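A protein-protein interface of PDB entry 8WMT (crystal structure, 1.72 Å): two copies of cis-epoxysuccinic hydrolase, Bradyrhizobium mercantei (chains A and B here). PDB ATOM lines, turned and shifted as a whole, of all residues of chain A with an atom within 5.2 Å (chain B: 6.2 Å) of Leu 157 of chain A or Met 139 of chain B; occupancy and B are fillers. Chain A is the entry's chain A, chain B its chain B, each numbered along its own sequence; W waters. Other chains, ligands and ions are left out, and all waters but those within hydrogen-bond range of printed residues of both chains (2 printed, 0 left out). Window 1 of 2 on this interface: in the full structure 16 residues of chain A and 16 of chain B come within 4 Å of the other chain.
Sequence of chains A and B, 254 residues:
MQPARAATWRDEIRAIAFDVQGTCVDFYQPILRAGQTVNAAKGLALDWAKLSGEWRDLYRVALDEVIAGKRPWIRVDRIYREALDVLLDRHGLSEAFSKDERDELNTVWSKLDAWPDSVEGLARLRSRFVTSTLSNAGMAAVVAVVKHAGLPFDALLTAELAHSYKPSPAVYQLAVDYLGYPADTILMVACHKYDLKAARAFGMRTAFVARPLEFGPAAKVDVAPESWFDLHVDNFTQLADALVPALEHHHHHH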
ATOM      1  N   SER A 132     -29.975  -5.560  21.379  1.00  0.00           N
ATOM      2  CA  SER A 132     -29.091  -5.761  22.518  1.00  0.00           C
ATOM      3  C   SER A 132     -28.628  -4.409  23.052  1.00  0.00           C
ATOM      4  O   SER A 132     -28.537  -3.427  22.312  1.00  0.00           O
ATOM      5  CB  SER A 132     -27.865  -6.598  22.108  1.00  0.00           C
ATOM      6  OG  SER A 132     -27.032  -6.905  23.223  1.00  0.00           O
ATOM      7  N   THR A 133     -28.345  -4.356  24.345  1.00  0.00           N
ATOM      8  CA  THR A 133     -27.557  -3.245  24.834  1.00  0.00           C
ATOM      9  C   THR A 133     -26.082  -3.476  24.497  1.00  0.00           C
ATOM     10  O   THR A 133     -25.631  -4.603  24.310  1.00  0.00           O
ATOM     11  CB  THR A 133     -27.711  -3.070  26.351  1.00  0.00           C
ATOM     12  OG1 THR A 133     -27.086  -4.160  27.033  1.00  0.00           O
ATOM     13  CG2 THR A 133     -29.208  -3.011  26.753  1.00  0.00           C
ATOM     14  N   LEU A 134     -25.336  -2.380  24.417  1.00  0.00           N
ATOM     15  CA  LEU A 134     -23.876  -2.457  24.372  1.00  0.00           C
ATOM     16  C   LEU A 134     -23.376  -1.126  24.930  1.00  0.00           C
ATOM     17  O   LEU A 134     -23.214  -0.155  24.193  1.00  0.00           O
ATOM     18  CB  LEU A 134     -23.350  -2.712  22.963  1.00  0.00           C
ATOM     19  CG  LEU A 134     -21.821  -2.971  22.907  1.00  0.00           C
ATOM     20  CD1 LEU A 134     -21.452  -4.301  23.571  1.00  0.00           C
ATOM     21  CD2 LEU A 134     -21.324  -2.938  21.456  1.00  0.00           C
ATOM     22  N   SER A 135     -23.153  -1.082  26.240  1.00  0.00           N
ATOM     23  CA  SER A 135     -22.792   0.181  26.869  1.00  0.00           C
ATOM     24  C   SER A 135     -21.582  -0.015  27.772  1.00  0.00           C
ATOM     25  O   SER A 135     -21.124  -1.130  28.001  1.00  0.00           O
ATOM     26  CB  SER A 135     -23.981   0.773  27.638  1.00  0.00           C
ATOM     27  OG  SER A 135     -24.142   0.155  28.896  1.00  0.00           O
ATOM     28  N   MET A 139     -22.637  -4.631  34.128  1.00  0.00           N
ATOM     29  CA  MET A 139     -23.747  -5.515  33.776  1.00  0.00           C
ATOM     30  C   MET A 139     -24.895  -5.362  34.767  1.00  0.00           C
ATOM     31  O   MET A 139     -26.054  -5.222  34.370  1.00  0.00           O
ATOM     32  CB  MET A 139     -23.290  -6.974  33.733  1.00  0.00           C
ATOM     33  CG  MET A 139     -22.523  -7.374  32.461  1.00  0.00           C
ATOM     34  SD  MET A 139     -23.567  -7.552  30.990  1.00  0.00           S
ATOM     35  CE  MET A 139     -24.323  -9.168  31.277  1.00  0.00           C
ATOM     36  N   ALA A 155     -31.054  -9.058  24.458  1.00  0.00           N
ATOM     37  CA  ALA A 155     -29.823  -9.389  25.169  1.00  0.00           C
ATOM     38  C   ALA A 155     -29.287  -8.144  25.861  1.00  0.00           C
ATOM     39  O   ALA A 155     -29.516  -7.023  25.407  1.00  0.00           O
ATOM     40  CB  ALA A 155     -28.749  -9.953  24.222  1.00  0.00           C
ATOM     41  N   LEU A 156     -28.559  -8.356  26.955  1.00  0.00           N
ATOM     42  CA  LEU A 156     -27.908  -7.265  27.673  1.00  0.00           C
ATOM     43  C   LEU A 156     -26.412  -7.532  27.703  1.00  0.00           C
ATOM     44  O   LEU A 156     -25.958  -8.445  28.399  1.00  0.00           O
ATOM     45  CB  LEU A 156     -28.427  -7.119  29.106  1.00  0.00           C
ATOM     46  CG  LEU A 156     -29.613  -6.189  29.356  1.00  0.00           C
ATOM     47  CD1 LEU A 156     -30.793  -6.480  28.434  1.00  0.00           C
ATOM     48  CD2 LEU A 156     -30.004  -6.136  30.830  1.00  0.00           C
ATOM     49  N   LEU A 157     -25.654  -6.718  26.977  1.00  0.00           N
ATOM     50  CA  LEU A 157     -24.199  -6.791  26.930  1.00  0.00           C
ATOM     51  C   LEU A 157     -23.612  -5.470  27.386  1.00  0.00           C
ATOM     52  O   LEU A 157     -24.170  -4.408  27.100  1.00  0.00           O
ATOM     53  CB  LEU A 157     -23.687  -7.076  25.503  1.00  0.00           C
ATOM     54  CG  LEU A 157     -24.293  -8.293  24.817  1.00  0.00           C
ATOM     55  CD1 LEU A 157     -23.744  -8.397  23.384  1.00  0.00           C
ATOM     56  CD2 LEU A 157     -23.966  -9.553  25.612  1.00  0.00           C
ATOM     57  N   THR A 158     -22.469  -5.524  28.073  1.00  0.00           N
ATOM     58  CA  THR A 158     -21.782  -4.296  28.437  1.00  0.00           C
ATOM     59  C   THR A 158     -20.283  -4.510  28.370  1.00  0.00           C
ATOM     60  O   THR A 158     -19.791  -5.645  28.375  1.00  0.00           O
ATOM     61  CB  THR A 158     -22.133  -3.768  29.850  1.00  0.00           C
ATOM     62  OG1 THR A 158     -21.336  -4.428  30.838  1.00  0.00           O
ATOM     63  CG2 THR A 158     -23.640  -3.917  30.191  1.00  0.00           C
ATOM     64  N   ALA A 159     -19.560  -3.385  28.381  1.00  0.00           N
ATOM     65  CA  ALA A 159     -18.102  -3.422  28.353  1.00  0.00           C
ATOM     66  C   ALA A 159     -17.503  -4.191  29.522  1.00  0.00           C
ATOM     67  O   ALA A 159     -16.352  -4.635  29.421  1.00  0.00           O
ATOM     68  CB  ALA A 159     -17.544  -1.989  28.323  1.00  0.00           C
ATOM     69  N   LEU A 161     -17.986  -7.098  30.209  1.00  0.00           N
ATOM     70  CA  LEU A 161     -17.686  -8.444  29.729  1.00  0.00           C
ATOM     71  C   LEU A 161     -16.329  -8.520  29.046  1.00  0.00           C
ATOM     72  O   LEU A 161     -15.840  -9.628  28.795  1.00  0.00           O
ATOM     73  CB  LEU A 161     -18.782  -8.920  28.771  1.00  0.00           C
ATOM     74  CG  LEU A 161     -20.214  -8.900  29.327  1.00  0.00           C
ATOM     75  CD1 LEU A 161     -21.212  -9.302  28.244  1.00  0.00           C
ATOM     76  CD2 LEU A 161     -20.318  -9.826  30.547  1.00  0.00           C
ATOM     77  N   LEU A 174     -17.800  -8.060  21.492  1.00  0.00           N
ATOM     78  CA  LEU A 174     -18.801  -8.742  22.313  1.00  0.00           C
ATOM     79  C   LEU A 174     -20.101  -8.951  21.551  1.00  0.00           C
ATOM     80  O   LEU A 174     -20.733 -10.010  21.664  1.00  0.00           O
ATOM     81  CB  LEU A 174     -19.101  -7.949  23.588  1.00  0.00           C
ATOM     82  CG  LEU A 174     -17.935  -7.659  24.516  1.00  0.00           C
ATOM     83  CD1 LEU A 174     -18.392  -6.630  25.555  1.00  0.00           C
ATOM     84  CD2 LEU A 174     -17.417  -8.943  25.166  1.00  0.00           C
ATOM     85  N   ALA A 175     -20.552  -7.931  20.822  1.00  0.00           N
ATOM     86  CA  ALA A 175     -21.804  -8.050  20.088  1.00  0.00           C
ATOM     87  C   ALA A 175     -21.689  -9.097  18.989  1.00  0.00           C
ATOM     88  O   ALA A 175     -22.615  -9.882  18.760  1.00  0.00           O
ATOM     89  CB  ALA A 175     -22.194  -6.690  19.518  1.00  0.00           C
ATOM     90  N   TYR A 178     -21.356 -12.644  20.944  1.00  0.00           N
ATOM     91  CA  TYR A 178     -22.435 -13.057  21.832  1.00  0.00           C
ATOM     92  C   TYR A 178     -23.823 -12.876  21.233  1.00  0.00           C
ATOM     93  O   TYR A 178     -24.782 -13.471  21.747  1.00  0.00           O
ATOM     94  CB  TYR A 178     -22.329 -12.302  23.171  1.00  0.00           C
ATOM     95  CG  TYR A 178     -21.089 -12.641  23.964  1.00  0.00           C
ATOM     96  CD1 TYR A 178     -20.441 -13.860  23.797  1.00  0.00           C
ATOM     97  CD2 TYR A 178     -20.558 -11.742  24.898  1.00  0.00           C
ATOM     98  CE1 TYR A 178     -19.292 -14.177  24.530  1.00  0.00           C
ATOM     99  CE2 TYR A 178     -19.434 -12.058  25.634  1.00  0.00           C
ATOM    100  CZ  TYR A 178     -18.798 -13.269  25.449  1.00  0.00           C
ATOM    101  OH  TYR A 178     -17.668 -13.565  26.196  1.00  0.00           O
ATOM    102  N   LEU A 179     -23.966 -12.093  20.166  1.00  0.00           N
ATOM    103  CA  LEU A 179     -25.197 -12.134  19.384  1.00  0.00           C
ATOM    104  C   LEU A 179     -25.092 -13.065  18.180  1.00  0.00           C
ATOM    105  O   LEU A 179     -26.121 -13.562  17.707  1.00  0.00           O
ATOM    106  CB  LEU A 179     -25.593 -10.729  18.917  1.00  0.00           C
ATOM    107  CG  LEU A 179     -25.647  -9.649  20.008  1.00  0.00           C
ATOM    108  CD1 LEU A 179     -26.001  -8.258  19.428  1.00  0.00           C
ATOM    109  CD2 LEU A 179     -26.655 -10.059  21.120  1.00  0.00           C
ATOM    110  N   ARG B  75     -17.478 -24.028  22.213  1.00  0.00           N
ATOM    111  CA  ARG B  75     -18.876 -23.653  22.409  1.00  0.00           C
ATOM    112  C   ARG B  75     -19.814 -24.845  22.206  1.00  0.00           C
ATOM    113  O   ARG B  75     -19.546 -25.745  21.409  1.00  0.00           O
ATOM    114  CB  ARG B  75     -19.239 -22.543  21.428  1.00  0.00           C
ATOM    115  CG  ARG B  75     -20.139 -21.458  21.967  1.00  0.00           C
ATOM    116  CD  ARG B  75     -20.183 -20.286  21.006  1.00  0.00           C
ATOM    117  NE  ARG B  75     -20.649 -20.687  19.686  1.00  0.00           N
ATOM    118  CZ  ARG B  75     -20.615 -19.902  18.617  1.00  0.00           C
ATOM    119  NH1 ARG B  75     -20.132 -18.672  18.681  1.00  0.00           N
ATOM    120  NH2 ARG B  75     -21.088 -20.359  17.458  1.00  0.00           N
ATOM    121  N   ALA B 137     -25.074 -23.324  27.306  1.00  0.00           N
ATOM    122  CA  ALA B 137     -25.002 -23.069  25.875  1.00  0.00           C
ATOM    123  C   ALA B 137     -24.354 -21.712  25.595  1.00  0.00           C
ATOM    124  O   ALA B 137     -24.230 -20.861  26.477  1.00  0.00           O
ATOM    125  CB  ALA B 137     -26.398 -23.135  25.250  1.00  0.00           C
ATOM    126  N   GLY B 138     -23.925 -21.519  24.349  1.00  0.00           N
ATOM    127  CA  GLY B 138     -23.325 -20.248  23.976  1.00  0.00           C
ATOM    128  C   GLY B 138     -24.314 -19.103  24.101  1.00  0.00           C
ATOM    129  O   GLY B 138     -25.528 -19.289  23.985  1.00  0.00           O
ATOM    130  N   MET B 139     -23.776 -17.898  24.318  1.00  0.00           N
ATOM    131  CA  MET B 139     -24.629 -16.708  24.435  1.00  0.00           C
ATOM    132  C   MET B 139     -25.524 -16.529  23.208  1.00  0.00           C
ATOM    133  O   MET B 139     -26.724 -16.254  23.329  1.00  0.00           O
ATOM    134  CB  MET B 139     -23.766 -15.459  24.642  1.00  0.00           C
ATOM    135  CG  MET B 139     -23.156 -15.329  26.034  1.00  0.00           C
ATOM    136  SD  MET B 139     -24.410 -14.782  27.240  1.00  0.00           S
ATOM    137  CE  MET B 139     -24.631 -13.075  26.697  1.00  0.00           C
ATOM    138  N   ALA B 140     -24.958 -16.663  22.005  1.00  0.00           N
ATOM    139  CA  ALA B 140     -25.746 -16.391  20.804  1.00  0.00           C
ATOM    140  C   ALA B 140     -26.886 -17.390  20.650  1.00  0.00           C
ATOM    141  O   ALA B 140     -27.988 -17.036  20.206  1.00  0.00           O
ATOM    142  CB  ALA B 140     -24.847 -16.417  19.567  1.00  0.00           C
ATOM    143  N   ALA B 141     -26.635 -18.644  21.016  1.00  0.00           N
ATOM    144  CA  ALA B 141     -27.679 -19.656  20.928  1.00  0.00           C
ATOM    145  C   ALA B 141     -28.789 -19.378  21.932  1.00  0.00           C
ATOM    146  O   ALA B 141     -29.975 -19.509  21.609  1.00  0.00           O
ATOM    147  CB  ALA B 141     -27.069 -21.041  21.156  1.00  0.00           C
ATOM    148  N   VAL B 142     -28.423 -18.965  23.145  1.00  0.00           N
ATOM    149  CA  VAL B 142     -29.441 -18.702  24.157  1.00  0.00           C
ATOM    150  C   VAL B 142     -30.226 -17.445  23.800  1.00  0.00           C
ATOM    151  O   VAL B 142     -31.446 -17.395  23.990  1.00  0.00           O
ATOM    152  CB  VAL B 142     -28.812 -18.620  25.560  1.00  0.00           C
ATOM    153  CG1 VAL B 142     -29.851 -18.157  26.578  1.00  0.00           C
ATOM    154  CG2 VAL B 142     -28.271 -20.000  25.972  1.00  0.00           C
ATOM    155  N   VAL B 143     -29.559 -16.425  23.249  1.00  0.00           N
ATOM    156  CA  VAL B 143     -30.285 -15.258  22.744  1.00  0.00           C
ATOM    157  C   VAL B 143     -31.339 -15.697  21.732  1.00  0.00           C
ATOM    158  O   VAL B 143     -32.500 -15.269  21.784  1.00  0.00           O
ATOM    159  CB  VAL B 143     -29.315 -14.235  22.117  1.00  0.00           C
ATOM    160  CG1 VAL B 143     -30.080 -13.220  21.290  1.00  0.00           C
ATOM    161  CG2 VAL B 143     -28.502 -13.525  23.179  1.00  0.00           C
ATOM    162  N   ALA B 144     -30.947 -16.582  20.807  1.00  0.00           N
ATOM    163  CA  ALA B 144     -31.883 -17.030  19.778  1.00  0.00           C
ATOM    164  C   ALA B 144     -32.999 -17.884  20.366  1.00  0.00           C
ATOM    165  O   ALA B 144     -34.164 -17.727  19.986  1.00  0.00           O
ATOM    166  CB  ALA B 144     -31.132 -17.805  18.693  1.00  0.00           C
ATOM    167  N   LEU B 156     -29.607 -12.219  30.245  1.00  0.00           N
ATOM    168  CA  LEU B 156     -29.207 -13.455  29.569  1.00  0.00           C
ATOM    169  C   LEU B 156     -27.732 -13.717  29.849  1.00  0.00           C
ATOM    170  O   LEU B 156     -26.857 -13.024  29.313  1.00  0.00           O
ATOM    171  CB  LEU B 156     -29.471 -13.375  28.062  1.00  0.00           C
ATOM    172  CG  LEU B 156     -30.678 -14.163  27.568  1.00  0.00           C
ATOM    173  CD1 LEU B 156     -31.956 -13.648  28.214  1.00  0.00           C
ATOM    174  CD2 LEU B 156     -30.806 -14.136  26.057  1.00  0.00           C
ATOM    175  N   LEU B 157     -27.456 -14.696  30.703  1.00  0.00           N
ATOM    176  CA  LEU B 157     -26.098 -15.109  31.026  1.00  0.00           C
ATOM    177  C   LEU B 157     -25.908 -16.568  30.647  1.00  0.00           C
ATOM    178  O   LEU B 157     -26.834 -17.381  30.750  1.00  0.00           O
ATOM    179  CB  LEU B 157     -25.798 -14.933  32.518  1.00  0.00           C
ATOM    180  CG  LEU B 157     -26.133 -13.575  33.132  1.00  0.00           C
ATOM    181  CD1 LEU B 157     -25.907 -13.598  34.659  1.00  0.00           C
ATOM    182  CD2 LEU B 157     -25.318 -12.447  32.456  1.00  0.00           C
ATOM    183  N   THR B 158     -24.701 -16.913  30.197  1.00  0.00           N
ATOM    184  CA  THR B 158     -24.384 -18.319  29.996  1.00  0.00           C
ATOM    185  C   THR B 158     -22.939 -18.591  30.388  1.00  0.00           C
ATOM    186  O   THR B 158     -22.131 -17.681  30.587  1.00  0.00           O
ATOM    187  CB  THR B 158     -24.571 -18.806  28.543  1.00  0.00           C
ATOM    188  OG1 THR B 158     -23.401 -18.488  27.771  1.00  0.00           O
ATOM    189  CG2 THR B 158     -25.814 -18.221  27.864  1.00  0.00           C
ATOM    190  N   GLU B 160     -20.572 -19.392  28.655  1.00  0.00           N
ATOM    191  CA  GLU B 160     -19.572 -18.878  27.721  1.00  0.00           C
ATOM    192  C   GLU B 160     -18.887 -17.639  28.287  1.00  0.00           C
ATOM    193  O   GLU B 160     -17.709 -17.371  27.988  1.00  0.00           O
ATOM    194  CB  GLU B 160     -20.216 -18.551  26.367  1.00  0.00           C
ATOM    195  CG  GLU B 160     -19.201 -17.963  25.373  1.00  0.00           C
ATOM    196  CD  GLU B 160     -19.741 -17.729  23.977  1.00  0.00           C
ATOM    197  OE1 GLU B 160     -20.962 -17.855  23.748  1.00  0.00           O
ATOM    198  OE2 GLU B 160     -18.912 -17.531  23.061  1.00  0.00           O
ATOM    199  N   LEU B 161     -19.603 -16.879  29.126  1.00  0.00           N
ATOM    200  CA  LEU B 161     -19.023 -15.686  29.731  1.00  0.00           C
ATOM    201  C   LEU B 161     -17.901 -16.018  30.702  1.00  0.00           C
ATOM    202  O   LEU B 161     -17.127 -15.122  31.066  1.00  0.00           O
ATOM    203  CB  LEU B 161     -20.102 -14.879  30.461  1.00  0.00           C
ATOM    204  CG  LEU B 161     -21.237 -14.439  29.547  1.00  0.00           C
ATOM    205  CD1 LEU B 161     -22.304 -13.729  30.378  1.00  0.00           C
ATOM    206  CD2 LEU B 161     -20.731 -13.529  28.442  1.00  0.00           C
HETATM  207  O   HOH W   1     -27.747 -10.505  28.825  1.00  0.00           O
HETATM  208  O   HOH W   2     -28.327 -15.054  18.452  1.00  0.00           O
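Water W2 lies within hydrogen-bond range of the backbone carbonyl oxygen of Ala 140 of chain B (2.7 Å) and the backbone carbonyl oxygen of Leu 179 of chain A (2.8 Å).
Water W1 bridges the backbone carbonyl oxygen (O) of Leu 156 of chain B (2.7 Å) and the backbone carbonyl oxygen (O) of Leu 156 of chain A (2.8 Å).
Among the printed residues, pairs that only touch across the chains: Met 139 of chain A with Leu 157 of chain B (3.6 Å), Ala 155 of chain A with Val 143 of chain B (3.7 Å), Leu 157 of chain A with Met 139 of chain B (3.7 Å), Tyr 178 of chain A with Met 139 of chain B (3.5 Å), Tyr 178 of chain A with Val 143 of chain B (3.99 Å), Tyr 178 of chain A with Glu 160 of chain B (3.6 Å), Tyr 178 of chain A with Leu 161 of chain B (3.4 Å) and Leu 179 of chain A with Ala 140 of chain B (3.6 Å).
Met 139 of chain A touches Leu 157 of chain B, and with the chains exchanged Leu 157 of chain A touches Met 139 of chain B.
Positions printed for both chains: 139, 156, 157, 158 and 161.
Of the 9 pairs that touch across the chains among the printed residues, 2 have their exchanged pair printed and touching as well.
The side-chain hydroxyl (OG) of Ser 132 of chain A lies close to the backbone carbonyl oxygen (O) of Ala 155 of chain A, 3.3 Å away.
O of Ala 155 of chain A sits at hydrogen-bond distance from N of Thr 133 of chain A (3.1 Å).
The side-chain hydroxyl (OG1) of Thr 133 of chain A sits at hydrogen-bond distance from the backbone carbonyl oxygen (O) of Leu 157 of chain A, at 2.9 Å.
The side-chain sulfur (SD) of Met 139 of chain B sits at hydrogen-bond distance from the backbone NH (N) of Thr 158 of chain B.
N of Met 139 of chain B sits at hydrogen-bond distance from OE1 of Glu 160 of chain B, 2.9 Å away.
The side-chain hydroxyl (OG1) of Thr 158 of chain B lies close to the backbone NH (N) of Glu 160 of chain B (3.1 Å).
The backbone carbonyl oxygen of Tyr 178 of chain A lies within hydrogen-bond range of the backbone NH of Ala 140 of chain B (3.2 Å).
Of the 15 printed residues of chain A, 5 touch a printed residue of chain B.
Hydrophobic or aromatic side chains of chain A within 4 Å of the printed part of chain B: Met 139, Ala 155, Leu 157 and Tyr 178.
Hydrophobic or aromatic side chains of chain B within 4 Å of the printed part of chain A: Met 139, Ala 140, Val 143, Leu 157 and Leu 161.
Among the printed residues, no Asp or Glu carboxylate lies within 4 Å of a Lys or Arg side-chain nitrogen of the other chain.
Ser 132 of chain A touches none of the printed residues of chain B.
Of the printed residues of chain B, Ala 155 of chain A touches Val 143.
Leu 157 of chain A touches one residue of chain B.
Leu 161 of chain A touches none of the printed residues of chain B.
Of the printed residues of chain B, Tyr 178 of chain A touches Met 139, Ala 140, Val 143, Glu 160 and Leu 161.
Of the printed residues of chain B, Leu 179 of chain A touches Ala 140.
Met 139 of chain B touches two residues of chain A.
Printed residues of chain A within 4 Å of Val 143 of chain B: Ala 155 (3.7 Å) and Tyr 178 (3.99 Å).
Printed residues of chain A within 4 Å of Leu 161 of chain B: Tyr 178 (3.4 Å).
The nearest printed residue of chain B that does not touch Leu 157 of chain A is Leu 156 of chain B (5.8 Å).
The nearest residue of chain A that does not touch Met 139 of chain B is Leu 156 of chain A (5.1 Å).
The nearest printed residue of chain A that does not touch Glu 160 of chain B is Leu 179 of chain A (7.4 Å).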
